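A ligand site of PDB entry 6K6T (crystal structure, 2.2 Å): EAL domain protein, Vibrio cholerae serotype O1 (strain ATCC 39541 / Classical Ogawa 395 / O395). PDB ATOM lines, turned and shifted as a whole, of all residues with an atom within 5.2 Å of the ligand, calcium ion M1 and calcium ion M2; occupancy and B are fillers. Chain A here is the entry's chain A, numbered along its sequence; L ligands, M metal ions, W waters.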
ATOM      1  N   MET A  28      30.835 -10.512  16.857  1.00  0.00           N
ATOM      2  CA  MET A  28      29.918  -9.664  17.614  1.00  0.00           C
ATOM      3  C   MET A  28      28.466 -10.091  17.469  1.00  0.00           C
ATOM      4  O   MET A  28      28.049 -10.608  16.427  1.00  0.00           O
ATOM      5  CB  MET A  28      30.048  -8.193  17.176  1.00  0.00           C
ATOM      6  CG  MET A  28      31.358  -7.542  17.563  1.00  0.00           C
ATOM      7  SD  MET A  28      31.576  -7.294  19.346  1.00  0.00           S
ATOM      8  CE  MET A  28      33.294  -6.818  19.446  1.00  0.00           C
ATOM      9  N   GLN A  31      22.330  -5.883  19.753  1.00  0.00           N
ATOM     10  CA  GLN A  31      21.017  -5.792  20.411  1.00  0.00           C
ATOM     11  C   GLN A  31      20.418  -4.414  20.192  1.00  0.00           C
ATOM     12  O   GLN A  31      21.044  -3.403  20.512  1.00  0.00           O
ATOM     13  CB  GLN A  31      21.089  -6.101  21.916  1.00  0.00           C
ATOM     14  CG  GLN A  31      19.708  -6.193  22.559  1.00  0.00           C
ATOM     15  CD  GLN A  31      19.728  -6.575  24.056  1.00  0.00           C
ATOM     16  OE1 GLN A  31      20.658  -6.242  24.775  1.00  0.00           O
ATOM     17  NE2 GLN A  31      18.709  -7.286  24.491  1.00  0.00           N
ATOM     18  N   GLU A  45      23.693  -2.037  20.374  1.00  0.00           N
ATOM     19  CA  GLU A  45      24.885  -2.270  21.166  1.00  0.00           C
ATOM     20  C   GLU A  45      25.605  -3.479  20.612  1.00  0.00           C
ATOM     21  O   GLU A  45      24.987  -4.517  20.377  1.00  0.00           O
ATOM     22  CB  GLU A  45      24.520  -2.510  22.638  1.00  0.00           C
ATOM     23  CG  GLU A  45      25.728  -2.616  23.529  1.00  0.00           C
ATOM     24  CD  GLU A  45      25.375  -2.913  24.987  1.00  0.00           C
ATOM     25  OE1 GLU A  45      24.179  -2.937  25.370  1.00  0.00           O
ATOM     26  OE2 GLU A  45      26.322  -3.154  25.764  1.00  0.00           O
ATOM     27  N   ALA A  46      26.922  -3.366  20.446  1.00  0.00           N
ATOM     28  CA  ALA A  46      27.734  -4.515  20.095  1.00  0.00           C
ATOM     29  C   ALA A  46      28.108  -5.343  21.320  1.00  0.00           C
ATOM     30  O   ALA A  46      28.522  -4.799  22.359  1.00  0.00           O
ATOM     31  CB  ALA A  46      29.016  -4.071  19.367  1.00  0.00           C
ATOM     32  N   LEU A  47      27.981  -6.658  21.194  1.00  0.00           N
ATOM     33  CA  LEU A  47      28.218  -7.575  22.310  1.00  0.00           C
ATOM     34  C   LEU A  47      29.051  -8.751  21.852  1.00  0.00           C
ATOM     35  O   LEU A  47      28.645  -9.463  20.937  1.00  0.00           O
ATOM     36  CB  LEU A  47      26.885  -8.080  22.916  1.00  0.00           C
ATOM     37  CG  LEU A  47      25.948  -6.988  23.479  1.00  0.00           C
ATOM     38  CD1 LEU A  47      24.547  -7.541  23.826  1.00  0.00           C
ATOM     39  CD2 LEU A  47      26.610  -6.305  24.681  1.00  0.00           C
ATOM     40  N   VAL A  48      30.174  -8.997  22.536  1.00  0.00           N
ATOM     41  CA  VAL A  48      31.119 -10.007  22.074  1.00  0.00           C
ATOM     42  C   VAL A  48      30.526 -11.400  22.225  1.00  0.00           C
ATOM     43  O   VAL A  48      29.794 -11.692  23.173  1.00  0.00           O
ATOM     44  CB  VAL A  48      32.471  -9.941  22.813  1.00  0.00           C
ATOM     45  CG1 VAL A  48      33.296  -8.812  22.309  1.00  0.00           C
ATOM     46  CG2 VAL A  48      32.257  -9.861  24.321  1.00  0.00           C
ATOM     47  N   ARG A  49      30.878 -12.255  21.277  1.00  0.00           N
ATOM     48  CA  ARG A  49      30.475 -13.652  21.236  1.00  0.00           C
ATOM     49  C   ARG A  49      31.645 -14.461  20.732  1.00  0.00           C
ATOM     50  O   ARG A  49      32.488 -13.948  19.981  1.00  0.00           O
ATOM     51  CB  ARG A  49      29.246 -13.888  20.330  1.00  0.00           C
ATOM     52  CG  ARG A  49      27.950 -13.248  20.836  1.00  0.00           C
ATOM     53  CD  ARG A  49      27.417 -13.927  22.100  1.00  0.00           C
ATOM     54  NE  ARG A  49      26.222 -13.263  22.628  1.00  0.00           N
ATOM     55  CZ  ARG A  49      26.257 -12.285  23.524  1.00  0.00           C
ATOM     56  NH1 ARG A  49      25.116 -11.724  23.948  1.00  0.00           N
ATOM     57  NH2 ARG A  49      27.412 -11.882  24.034  1.00  0.00           N
ATOM     58  N   ALA A  56      29.640 -13.865  25.980  1.00  0.00           N
ATOM     59  CA  ALA A  56      30.609 -12.780  26.088  1.00  0.00           C
ATOM     60  C   ALA A  56      31.620 -13.053  27.200  1.00  0.00           C
ATOM     61  O   ALA A  56      32.829 -12.909  26.998  1.00  0.00           O
ATOM     62  CB  ALA A  56      29.871 -11.452  26.333  1.00  0.00           C
ATOM     63  N   TYR A  57      31.141 -13.488  28.370  1.00  0.00           N
ATOM     64  CA  TYR A  57      32.025 -13.734  29.503  1.00  0.00           C
ATOM     65  C   TYR A  57      33.067 -14.789  29.168  1.00  0.00           C
ATOM     66  O   TYR A  57      34.247 -14.647  29.535  1.00  0.00           O
ATOM     67  CB  TYR A  57      31.204 -14.081  30.763  1.00  0.00           C
ATOM     68  CG  TYR A  57      31.202 -15.514  31.259  1.00  0.00           C
ATOM     69  CD1 TYR A  57      32.284 -16.043  31.971  1.00  0.00           C
ATOM     70  CD2 TYR A  57      30.077 -16.333  31.089  1.00  0.00           C
ATOM     71  CE1 TYR A  57      32.266 -17.364  32.456  1.00  0.00           C
ATOM     72  CE2 TYR A  57      30.043 -17.643  31.570  1.00  0.00           C
ATOM     73  CZ  TYR A  57      31.144 -18.157  32.255  1.00  0.00           C
ATOM     74  OH  TYR A  57      31.116 -19.445  32.726  1.00  0.00           O
ATOM     75  N   ILE A  60      35.582 -12.840  27.104  1.00  0.00           N
ATOM     76  CA  ILE A  60      36.265 -11.763  27.814  1.00  0.00           C
ATOM     77  C   ILE A  60      37.195 -12.294  28.892  1.00  0.00           C
ATOM     78  O   ILE A  60      38.231 -11.685  29.188  1.00  0.00           O
ATOM     79  CB  ILE A  60      35.220 -10.806  28.401  1.00  0.00           C
ATOM     80  CG1 ILE A  60      34.376 -10.195  27.276  1.00  0.00           C
ATOM     81  CG2 ILE A  60      35.870  -9.720  29.257  1.00  0.00           C
ATOM     82  CD1 ILE A  60      33.069  -9.631  27.753  1.00  0.00           C
ATOM     83  N   PHE A  71      42.884  -6.625  22.323  1.00  0.00           N
ATOM     84  CA  PHE A  71      41.496  -7.104  22.360  1.00  0.00           C
ATOM     85  C   PHE A  71      40.519  -5.941  22.282  1.00  0.00           C
ATOM     86  O   PHE A  71      39.469  -6.047  21.636  1.00  0.00           O
ATOM     87  CB  PHE A  71      41.247  -7.912  23.636  1.00  0.00           C
ATOM     88  CG  PHE A  71      39.795  -8.255  23.856  1.00  0.00           C
ATOM     89  CD1 PHE A  71      39.222  -9.332  23.212  1.00  0.00           C
ATOM     90  CD2 PHE A  71      39.006  -7.482  24.687  1.00  0.00           C
ATOM     91  CE1 PHE A  71      37.893  -9.660  23.398  1.00  0.00           C
ATOM     92  CE2 PHE A  71      37.665  -7.790  24.880  1.00  0.00           C
ATOM     93  CZ  PHE A  71      37.110  -8.879  24.230  1.00  0.00           C
ATOM     94  N   CYS A  75      37.912  -5.558  19.243  1.00  0.00           N
ATOM     95  CA  CYS A  75      36.494  -5.338  19.520  1.00  0.00           C
ATOM     96  C   CYS A  75      35.934  -4.197  18.697  1.00  0.00           C
ATOM     97  O   CYS A  75      34.880  -4.316  18.081  1.00  0.00           O
ATOM     98  CB  CYS A  75      36.273  -5.053  21.005  1.00  0.00           C
ATOM     99  SG  CYS A  75      35.880  -6.483  21.903  1.00  0.00           S
ATOM    100  N   ASN A  95      31.070  -1.163  23.954  1.00  0.00           N
ATOM    101  CA  ASN A  95      31.502  -1.186  25.340  1.00  0.00           C
ATOM    102  C   ASN A  95      32.981  -0.873  25.447  1.00  0.00           C
ATOM    103  O   ASN A  95      33.825  -1.591  24.892  1.00  0.00           O
ATOM    104  CB  ASN A  95      31.179  -2.539  25.963  1.00  0.00           C
ATOM    105  CG  ASN A  95      29.697  -2.707  26.258  1.00  0.00           C
ATOM    106  OD1 ASN A  95      29.183  -2.066  27.171  1.00  0.00           O
ATOM    107  ND2 ASN A  95      29.002  -3.534  25.479  1.00  0.00           N
ATOM    108  N   PHE A  96      33.289   0.187  26.175  1.00  0.00           N
ATOM    109  CA  PHE A  96      34.660   0.541  26.511  1.00  0.00           C
ATOM    110  C   PHE A  96      35.123  -0.401  27.619  1.00  0.00           C
ATOM    111  O   PHE A  96      34.530  -0.437  28.707  1.00  0.00           O
ATOM    112  CB  PHE A  96      34.713   2.001  26.930  1.00  0.00           C
ATOM    113  CG  PHE A  96      36.091   2.583  26.925  1.00  0.00           C
ATOM    114  CD1 PHE A  96      36.946   2.390  27.987  1.00  0.00           C
ATOM    115  CD2 PHE A  96      36.513   3.343  25.867  1.00  0.00           C
ATOM    116  CE1 PHE A  96      38.215   2.941  27.969  1.00  0.00           C
ATOM    117  CE2 PHE A  96      37.772   3.900  25.857  1.00  0.00           C
ATOM    118  CZ  PHE A  96      38.626   3.698  26.898  1.00  0.00           C
ATOM    119  N   LEU A  97      36.171  -1.170  27.340  1.00  0.00           N
ATOM    120  CA  LEU A  97      36.685  -2.110  28.316  1.00  0.00           C
ATOM    121  C   LEU A  97      37.059  -1.377  29.592  1.00  0.00           C
ATOM    122  O   LEU A  97      37.875  -0.437  29.540  1.00  0.00           O
ATOM    123  CB  LEU A  97      37.898  -2.858  27.776  1.00  0.00           C
ATOM    124  CG  LEU A  97      38.290  -4.121  28.548  1.00  0.00           C
ATOM    125  CD1 LEU A  97      37.159  -5.120  28.614  1.00  0.00           C
ATOM    126  CD2 LEU A  97      39.510  -4.754  27.921  1.00  0.00           C
ATOM    127  N   GLU A 128      30.350   3.174  25.732  1.00  0.00           N
ATOM    128  CA  GLU A 128      29.752   2.921  27.038  1.00  0.00           C
ATOM    129  C   GLU A 128      30.835   2.690  28.092  1.00  0.00           C
ATOM    130  O   GLU A 128      31.654   1.785  27.954  1.00  0.00           O
ATOM    131  CB  GLU A 128      28.795   1.712  26.971  1.00  0.00           C
ATOM    132  CG  GLU A 128      27.631   1.899  25.952  1.00  0.00           C
ATOM    133  CD  GLU A 128      26.561   0.831  26.025  1.00  0.00           C
ATOM    134  OE1 GLU A 128      25.689   0.807  25.137  1.00  0.00           O
ATOM    135  OE2 GLU A 128      26.570   0.009  26.970  1.00  0.00           O
ATOM    136  N   ASP A 158      27.344   3.343  31.515  1.00  0.00           N
ATOM    137  CA  ASP A 158      26.722   2.038  31.500  1.00  0.00           C
ATOM    138  C   ASP A 158      26.512   1.567  32.940  1.00  0.00           C
ATOM    139  O   ASP A 158      27.232   1.980  33.852  1.00  0.00           O
ATOM    140  CB  ASP A 158      27.605   1.042  30.745  1.00  0.00           C
ATOM    141  CG  ASP A 158      26.855  -0.200  30.296  1.00  0.00           C
ATOM    142  OD1 ASP A 158      25.603  -0.213  30.358  1.00  0.00           O
ATOM    143  OD2 ASP A 158      27.523  -1.193  29.913  1.00  0.00           O
ATOM    144  N   ASP A 159      25.537   0.689  33.137  1.00  0.00           N
ATOM    145  CA  ASP A 159      25.319   0.017  34.432  1.00  0.00           C
ATOM    146  C   ASP A 159      25.071   0.998  35.581  1.00  0.00           C
ATOM    147  O   ASP A 159      25.445   0.721  36.722  1.00  0.00           O
ATOM    148  CB  ASP A 159      26.524  -0.848  34.812  1.00  0.00           C
ATOM    149  CG  ASP A 159      26.774  -1.989  33.879  1.00  0.00           C
ATOM    150  OD1 ASP A 159      25.809  -2.548  33.319  1.00  0.00           O
ATOM    151  OD2 ASP A 159      27.963  -2.314  33.689  1.00  0.00           O
ATOM    152  N   LYS A 179      22.787   4.831  30.994  1.00  0.00           N
ATOM    153  CA  LYS A 179      22.056   3.574  30.900  1.00  0.00           C
ATOM    154  C   LYS A 179      21.775   3.069  32.324  1.00  0.00           C
ATOM    155  O   LYS A 179      22.680   2.667  33.050  1.00  0.00           O
ATOM    156  CB  LYS A 179      22.867   2.589  30.066  1.00  0.00           C
ATOM    157  CG  LYS A 179      23.212   3.133  28.653  1.00  0.00           C
ATOM    158  CD  LYS A 179      23.954   2.069  27.859  1.00  0.00           C
ATOM    159  CE  LYS A 179      22.976   1.195  27.100  1.00  0.00           C
ATOM    160  NZ  LYS A 179      23.615  -0.032  26.559  1.00  0.00           N
ATOM    161  N   ASP A 181      20.998   0.709  35.174  1.00  0.00           N
ATOM    162  CA  ASP A 181      21.224  -0.719  35.362  1.00  0.00           C
ATOM    163  C   ASP A 181      19.898  -1.475  35.491  1.00  0.00           C
ATOM    164  O   ASP A 181      18.928  -0.967  36.081  1.00  0.00           O
ATOM    165  CB  ASP A 181      22.080  -0.981  36.602  1.00  0.00           C
ATOM    166  CG  ASP A 181      22.535  -2.413  36.689  1.00  0.00           C
ATOM    167  OD1 ASP A 181      23.472  -2.743  35.917  1.00  0.00           O
ATOM    168  OD2 ASP A 181      21.989  -3.194  37.493  1.00  0.00           O
ATOM    169  N   MET A 182      19.869  -2.679  34.939  1.00  0.00           N
ATOM    170  CA  MET A 182      18.626  -3.422  34.851  1.00  0.00           C
ATOM    171  C   MET A 182      18.160  -3.924  36.212  1.00  0.00           C
ATOM    172  O   MET A 182      16.950  -4.127  36.398  1.00  0.00           O
ATOM    173  CB  MET A 182      18.751  -4.562  33.816  1.00  0.00           C
ATOM    174  CG  MET A 182      19.711  -5.681  34.166  1.00  0.00           C
ATOM    175  SD  MET A 182      19.743  -7.071  32.981  1.00  0.00           S
ATOM    176  CE  MET A 182      20.381  -6.215  31.535  1.00  0.00           C
ATOM    177  N   ARG A 186      14.119  -3.959  37.031  1.00  0.00           N
ATOM    178  CA  ARG A 186      13.422  -5.216  37.181  1.00  0.00           C
ATOM    179  C   ARG A 186      12.197  -5.026  38.069  1.00  0.00           C
ATOM    180  O   ARG A 186      12.299  -4.410  39.136  1.00  0.00           O
ATOM    181  CB  ARG A 186      14.359  -6.267  37.757  1.00  0.00           C
ATOM    182  CG  ARG A 186      13.731  -7.625  37.806  1.00  0.00           C
ATOM    183  CD  ARG A 186      13.427  -8.136  36.409  1.00  0.00           C
ATOM    184  NE  ARG A 186      14.640  -8.227  35.604  1.00  0.00           N
ATOM    185  CZ  ARG A 186      14.872  -7.559  34.477  1.00  0.00           C
ATOM    186  NH1 ARG A 186      13.967  -6.748  33.974  1.00  0.00           N
ATOM    187  NH2 ARG A 186      16.033  -7.742  33.841  1.00  0.00           N
ATOM    188  N   GLU A 215      17.682  -0.169  30.648  1.00  0.00           N
ATOM    189  CA  GLU A 215      18.306  -1.378  30.164  1.00  0.00           C
ATOM    190  C   GLU A 215      17.632  -2.626  30.771  1.00  0.00           C
ATOM    191  O   GLU A 215      17.042  -2.577  31.846  1.00  0.00           O
ATOM    192  CB  GLU A 215      19.788  -1.306  30.542  1.00  0.00           C
ATOM    193  CG  GLU A 215      20.671  -2.334  29.974  1.00  0.00           C
ATOM    194  CD  GLU A 215      22.116  -1.907  30.056  1.00  0.00           C
ATOM    195  OE1 GLU A 215      22.660  -1.810  31.173  1.00  0.00           O
ATOM    196  OE2 GLU A 215      22.655  -1.526  28.986  1.00  0.00           O
ATOM    197  N   GLY A 216      17.693  -3.740  30.039  1.00  0.00           N
ATOM    198  CA  GLY A 216      17.172  -4.979  30.579  1.00  0.00           C
ATOM    199  C   GLY A 216      15.668  -5.079  30.721  1.00  0.00           C
ATOM    200  O   GLY A 216      15.191  -5.838  31.561  1.00  0.00           O
ATOM    201  N   VAL A 217      14.898  -4.333  29.924  1.00  0.00           N
ATOM    202  CA  VAL A 217      13.440  -4.396  29.993  1.00  0.00           C
ATOM    203  C   VAL A 217      12.985  -5.758  29.495  1.00  0.00           C
ATOM    204  O   VAL A 217      13.262  -6.118  28.347  1.00  0.00           O
ATOM    205  CB  VAL A 217      12.785  -3.275  29.189  1.00  0.00           C
ATOM    206  CG1 VAL A 217      11.274  -3.407  29.219  1.00  0.00           C
ATOM    207  CG2 VAL A 217      13.156  -1.961  29.773  1.00  0.00           C
ATOM    208  N   GLU A 218      12.239  -6.499  30.344  1.00  0.00           N
ATOM    209  CA  GLU A 218      11.870  -7.871  30.063  1.00  0.00           C
ATOM    210  C   GLU A 218      10.380  -8.106  29.877  1.00  0.00           C
ATOM    211  O   GLU A 218      10.018  -9.145  29.310  1.00  0.00           O
ATOM    212  CB  GLU A 218      12.334  -8.816  31.202  1.00  0.00           C
ATOM    213  CG  GLU A 218      13.783  -9.310  31.092  1.00  0.00           C
ATOM    214  CD  GLU A 218      14.224 -10.156  32.262  1.00  0.00           C
ATOM    215  OE1 GLU A 218      15.409 -10.516  32.319  1.00  0.00           O
ATOM    216  OE2 GLU A 218      13.371 -10.475  33.112  1.00  0.00           O
ATOM    217  N   GLN A 235      16.072  -0.914  26.168  1.00  0.00           N
ATOM    218  CA  GLN A 235      16.791  -2.063  25.641  1.00  0.00           C
ATOM    219  C   GLN A 235      16.416  -3.267  26.490  1.00  0.00           C
ATOM    220  O   GLN A 235      16.208  -3.135  27.698  1.00  0.00           O
ATOM    221  CB  GLN A 235      18.305  -1.790  25.655  1.00  0.00           C
ATOM    222  CG  GLN A 235      19.170  -2.845  24.992  1.00  0.00           C
ATOM    223  CD  GLN A 235      20.651  -2.479  25.055  1.00  0.00           C
ATOM    224  OE1 GLN A 235      21.011  -1.304  25.160  1.00  0.00           O
ATOM    225  NE2 GLN A 235      21.503  -3.495  25.054  1.00  0.00           N
ATOM    226  N   GLY A 236      16.340  -4.428  25.852  1.00  0.00           N
ATOM    227  CA  GLY A 236      16.140  -5.649  26.618  1.00  0.00           C
ATOM    228  C   GLY A 236      15.414  -6.712  25.825  1.00  0.00           C
ATOM    229  O   GLY A 236      14.979  -6.515  24.686  1.00  0.00           O
ATOM    230  N   TYR A 237      15.315  -7.894  26.469  1.00  0.00           N
ATOM    231  CA  TYR A 237      14.716  -9.066  25.845  1.00  0.00           C
ATOM    232  C   TYR A 237      13.260  -8.821  25.443  1.00  0.00           C
ATOM    233  O   TYR A 237      12.774  -9.447  24.495  1.00  0.00           O
ATOM    234  CB  TYR A 237      14.779 -10.269  26.773  1.00  0.00           C
ATOM    235  CG  TYR A 237      16.169 -10.790  27.083  1.00  0.00           C
ATOM    236  CD1 TYR A 237      17.242 -10.449  26.283  1.00  0.00           C
ATOM    237  CD2 TYR A 237      16.382 -11.672  28.151  1.00  0.00           C
ATOM    238  CE1 TYR A 237      18.514 -10.955  26.554  1.00  0.00           C
ATOM    239  CE2 TYR A 237      17.635 -12.179  28.439  1.00  0.00           C
ATOM    240  CZ  TYR A 237      18.701 -11.819  27.625  1.00  0.00           C
ATOM    241  OH  TYR A 237      19.971 -12.311  27.895  1.00  0.00           O
ATOM    242  N   TYR A 238      12.557  -7.938  26.165  1.00  0.00           N
ATOM    243  CA  TYR A 238      11.209  -7.608  25.742  1.00  0.00           C
ATOM    244  C   TYR A 238      11.189  -7.157  24.292  1.00  0.00           C
ATOM    245  O   TYR A 238      10.302  -7.552  23.525  1.00  0.00           O
ATOM    246  CB  TYR A 238      10.595  -6.533  26.616  1.00  0.00           C
ATOM    247  CG  TYR A 238       9.207  -6.147  26.161  1.00  0.00           C
ATOM    248  CD1 TYR A 238       8.160  -7.076  26.159  1.00  0.00           C
ATOM    249  CD2 TYR A 238       8.921  -4.859  25.720  1.00  0.00           C
ATOM    250  CE1 TYR A 238       6.895  -6.732  25.745  1.00  0.00           C
ATOM    251  CE2 TYR A 238       7.644  -4.496  25.312  1.00  0.00           C
ATOM    252  CZ  TYR A 238       6.642  -5.432  25.311  1.00  0.00           C
ATOM    253  OH  TYR A 238       5.371  -5.060  24.904  1.00  0.00           O
ATOM    254  N   PRO A 242      19.910 -10.242  21.684  1.00  0.00           N
ATOM    255  CA  PRO A 242      20.968  -9.911  20.726  1.00  0.00           C
ATOM    256  C   PRO A 242      20.979 -10.920  19.575  1.00  0.00           C
ATOM    257  O   PRO A 242      20.676 -12.104  19.750  1.00  0.00           O
ATOM    258  CB  PRO A 242      22.252  -9.990  21.551  1.00  0.00           C
ATOM    259  CG  PRO A 242      21.801  -9.880  22.982  1.00  0.00           C
ATOM    260  CD  PRO A 242      20.440 -10.469  23.043  1.00  0.00           C
HETATM  261  C1  LIG L   1      22.151  -8.925  28.855  1.00  0.00           C
HETATM  262  C2  LIG L   1      30.700  -7.024  29.037  1.00  0.00           C
HETATM  263  C3  LIG L   1      18.473 -10.031  30.931  1.00  0.00           C
HETATM  264  C4  LIG L   1      22.982  -9.535  28.075  1.00  0.00           C
HETATM  265  C5  LIG L   1      33.923  -5.099  26.603  1.00  0.00           C
HETATM  266  C6  LIG L   1      29.835  -6.221  29.623  1.00  0.00           C
HETATM  267  C7  LIG L   1      24.440  -8.910  28.642  1.00  0.00           C
HETATM  268  C8  LIG L   1      28.467  -7.143  29.969  1.00  0.00           C
HETATM  269  C9  LIG L   1      19.733  -8.908  29.294  1.00  0.00           C
HETATM  270  C10 LIG L   1      24.300  -7.677  29.009  1.00  0.00           C
HETATM  271  C11 LIG L   1      31.979  -6.299  26.945  1.00  0.00           C
HETATM  272  C12 LIG L   1      28.613  -8.077  29.184  1.00  0.00           C
HETATM  273  C13 LIG L   1      18.624  -8.275  28.816  1.00  0.00           C
HETATM  274  C14 LIG L   1      24.831  -6.669  27.900  1.00  0.00           C
HETATM  275  C15 LIG L   1      31.821  -6.436  25.570  1.00  0.00           C
HETATM  276  C16 LIG L   1      27.718  -9.343  29.474  1.00  0.00           C
HETATM  277  C17 LIG L   1      17.394  -8.561  29.454  1.00  0.00           C
HETATM  278  C18 LIG L   1      32.795  -5.847  24.732  1.00  0.00           C
HETATM  279  C19 LIG L   1      20.357  -7.626  27.656  1.00  0.00           C
HETATM  280  C20 LIG L   1      30.181  -7.412  26.525  1.00  0.00           C
HETATM  281  N1  LIG L   1      17.380  -9.450  30.490  1.00  0.00           N
HETATM  282  N2  LIG L   1      33.806  -5.210  25.287  1.00  0.00           N
HETATM  283  N3  LIG L   1      19.651  -9.776  30.354  1.00  0.00           N
HETATM  284  N4  LIG L   1      33.036  -5.648  27.417  1.00  0.00           N
HETATM  285  N5  LIG L   1      19.051  -7.497  27.789  1.00  0.00           N
HETATM  286  N6  LIG L   1      30.697  -7.138  25.343  1.00  0.00           N
HETATM  287  N7  LIG L   1      20.767  -8.518  28.533  1.00  0.00           N
HETATM  288  N8  LIG L   1      30.928  -6.903  27.510  1.00  0.00           N
HETATM  289  O1  LIG L   1      26.529 -10.493  25.855  1.00  0.00           O
HETATM  290  O2  LIG L   1      25.851  -4.496  30.679  1.00  0.00           O
HETATM  291  O3  LIG L   1      22.886  -9.421  26.597  1.00  0.00           O
HETATM  292  O4  LIG L   1      25.823 -11.465  27.929  1.00  0.00           O
HETATM  293  O5  LIG L   1      29.503  -4.991  28.867  1.00  0.00           O
HETATM  294  O6  LIG L   1      27.357  -4.191  28.808  1.00  0.00           O
HETATM  295  O7  LIG L   1      25.341  -8.995  27.549  1.00  0.00           O
HETATM  296  O8  LIG L   1      27.079  -6.637  29.794  1.00  0.00           O
HETATM  297  O9  LIG L   1      22.766  -7.521  29.160  1.00  0.00           O
HETATM  298  O10 LIG L   1      30.176  -8.418  29.307  1.00  0.00           O
HETATM  299  O11 LIG L   1      25.154  -5.384  28.392  1.00  0.00           O
HETATM  300  O12 LIG L   1      27.743 -10.084  28.259  1.00  0.00           O
HETATM  301  O13 LIG L   1      16.185  -7.933  29.005  1.00  0.00           O
HETATM  302  O14 LIG L   1      32.689  -5.924  23.376  1.00  0.00           O
HETATM  303  P1  LIG L   1      26.391  -5.211  29.469  1.00  0.00           P
HETATM  304  P2  LIG L   1      26.411 -10.238  27.396  1.00  0.00           P
HETATM  305 CA    CA M   1      26.897  -2.027  27.793  1.00  0.00          CA
HETATM  306 CA    CA M   2      24.888  -2.429  31.188  1.00  0.00          CA
HETATM  307  O   HOH W   1      24.309  -5.876  33.160  1.00  0.00           O
HETATM  308  O   HOH W   2      27.009  -5.731  33.250  1.00  0.00           O
HETATM  309  O   HOH W   3      24.481  -2.319  27.994  1.00  0.00           O
HETATM  310  O   HOH W   4      30.960  -3.632  22.729  1.00  0.00           O
HETATM  311  O   HOH W   5      28.226 -12.510  29.038  1.00  0.00           O
HETATM  312  O   HOH W   6      28.539  -3.151  31.178  1.00  0.00           O
HETATM  313  O   HOH W   7      35.969  -3.538  24.494  1.00  0.00           O
HETATM  314  O   HOH W   8      19.340  -4.707  27.927  1.00  0.00           O
HETATM  315  O   HOH W   9      26.643 -14.041  26.564  1.00  0.00           O
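A nitrogen (N3) of the ligand is in hydrogen-bond range of the side-chain sulfur (SD) of Met 182, at 3.8 Å. An oxygen (O13) of the ligand sits at hydrogen-bond distance from the backbone NH (N) of Tyr 237, at 2.7 Å. The side-chain amide nitrogen (NE2) of Gln 31 lies within hydrogen-bond range of a nitrogen (N5) of the ligand, at 3.3 Å. N of Val 48 lies close to N6 of the ligand (3.4 Å). The side-chain carboxylate (OE1) of Glu 218 is in hydrogen-bond range of a nitrogen (N1) of the ligand, at 2.9 Å. SG of Cys 75 is in hydrogen-bond range of O14 of the ligand (3.6 Å). The guanidinium group of Arg 49 is in salt-bridge range of an oxygen (O1) of the ligand, 2.5 Å away.
N of Phe 96 lies within hydrogen-bond range of O of Glu 128 (2.9 Å). O of Gly 216 sits at hydrogen-bond distance from NH1 of Arg 186. The backbone NH of Asp 159 sits at hydrogen-bond distance from the backbone carbonyl oxygen of Lys 179 (3.5 Å). O of Gln 235 lies within hydrogen-bond range of N of Val 217. SG of Cys 75 sits close to O of Phe 71, 3.6 Å away. O of Val 217 lies within hydrogen-bond range of N of Tyr 238 (2.9 Å). The backbone NH of Gly 216 is in hydrogen-bond range of the backbone carbonyl oxygen of Gln 235 (2.8 Å). The side-chain amino group (NZ) of Lys 179 lies within salt-bridge range of the side-chain carboxylate (OE1) of Glu 128 (2.7 Å).
O13 of the ligand sits close to O of Gly 216. Leu 47 touches the ligand (CD2 to C14, 3.7 Å). Ala 56 touches the ligand (CB to O12, 3.2 Å). Ile 60 touches the ligand (CD1 to N8, 3.5 Å). CD1 of Leu 97 touches C5 of the ligand, at 3.8 Å. Arg 186 touches the ligand. O of Val 217 touches O13 of the ligand, 3.5 Å away. Gly 236 touches the ligand (CA to O13, 3.3 Å). Pro 242 touches the ligand (CG to O3, 3.8 Å). Hydrophobic or aromatic side chains that line the ligand: Leu 47, Val 48, Ala 56, Ile 60, Leu 97, Met 182, Tyr 237 and Pro 242. Of the 31 residues printed, 20 come within 4 Å of the ligand.
Within 4 Å of calcium ion M1: Glu 45, Asn 95, Glu 128 and Asp 158. The nearest printed residue that does not touch calcium ion M1 is Lys 179 (4.03 Å).
Within 4 Å of calcium ion M2: Asp 158, Asp 159 and Glu 215.
The side-chain carboxylate (OE2) of Glu 128 binds calcium ion M1. OD2 of Asp 158 binds calcium ion M1 (2.4 Å). OD1 of Asn 95 binds calcium ion M1, 2.4 Å away. Calcium ion M1 is bound by OE2 of Glu 45 (2.4 Å). Calcium ion M1 is bound by O6 of the ligand. Calcium ion M1 is bound by water W3 (2.4 Å). Calcium ion M1 has six donor atoms within binding distance.
OE1 of Glu 215 is bound to calcium ion M2 (2.3 Å). OD1 of Asp 159 binds calcium ion M2 (2.3 Å). O2 of the ligand binds calcium ion M2. OD1 of Asp 158 is bound to calcium ion M2, 2.5 Å away. Calcium ion M2 has four donor atoms within binding distance.
Water W3 lies within hydrogen-bond range of OE1 of Glu 45, NZ of Lys 179 and O11 of the ligand. Water W5 bridges an oxygen (O12) of the ligand (2.6 Å) and the backbone NH (N) of Tyr 57 (3.1 Å). Water W8 bridges a nitrogen (N5) of the ligand (2.8 Å) and the backbone NH of Gly 216 (2.8 Å). Water W7 lies within hydrogen-bond range of N2 of the ligand and O of Asn 95. Water W4 lies within hydrogen-bond range of the backbone carbonyl oxygen (O) of Ala 46, the backbone NH (N) of Asn 95 and an oxygen (O14) of the ligand. Water W9 lies within hydrogen-bond range of an oxygen (O4) of the ligand (3.0 Å), the backbone NH of Ala 56 (3.1 Å) and the guanidinium group of Arg 49 (3.4 Å).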
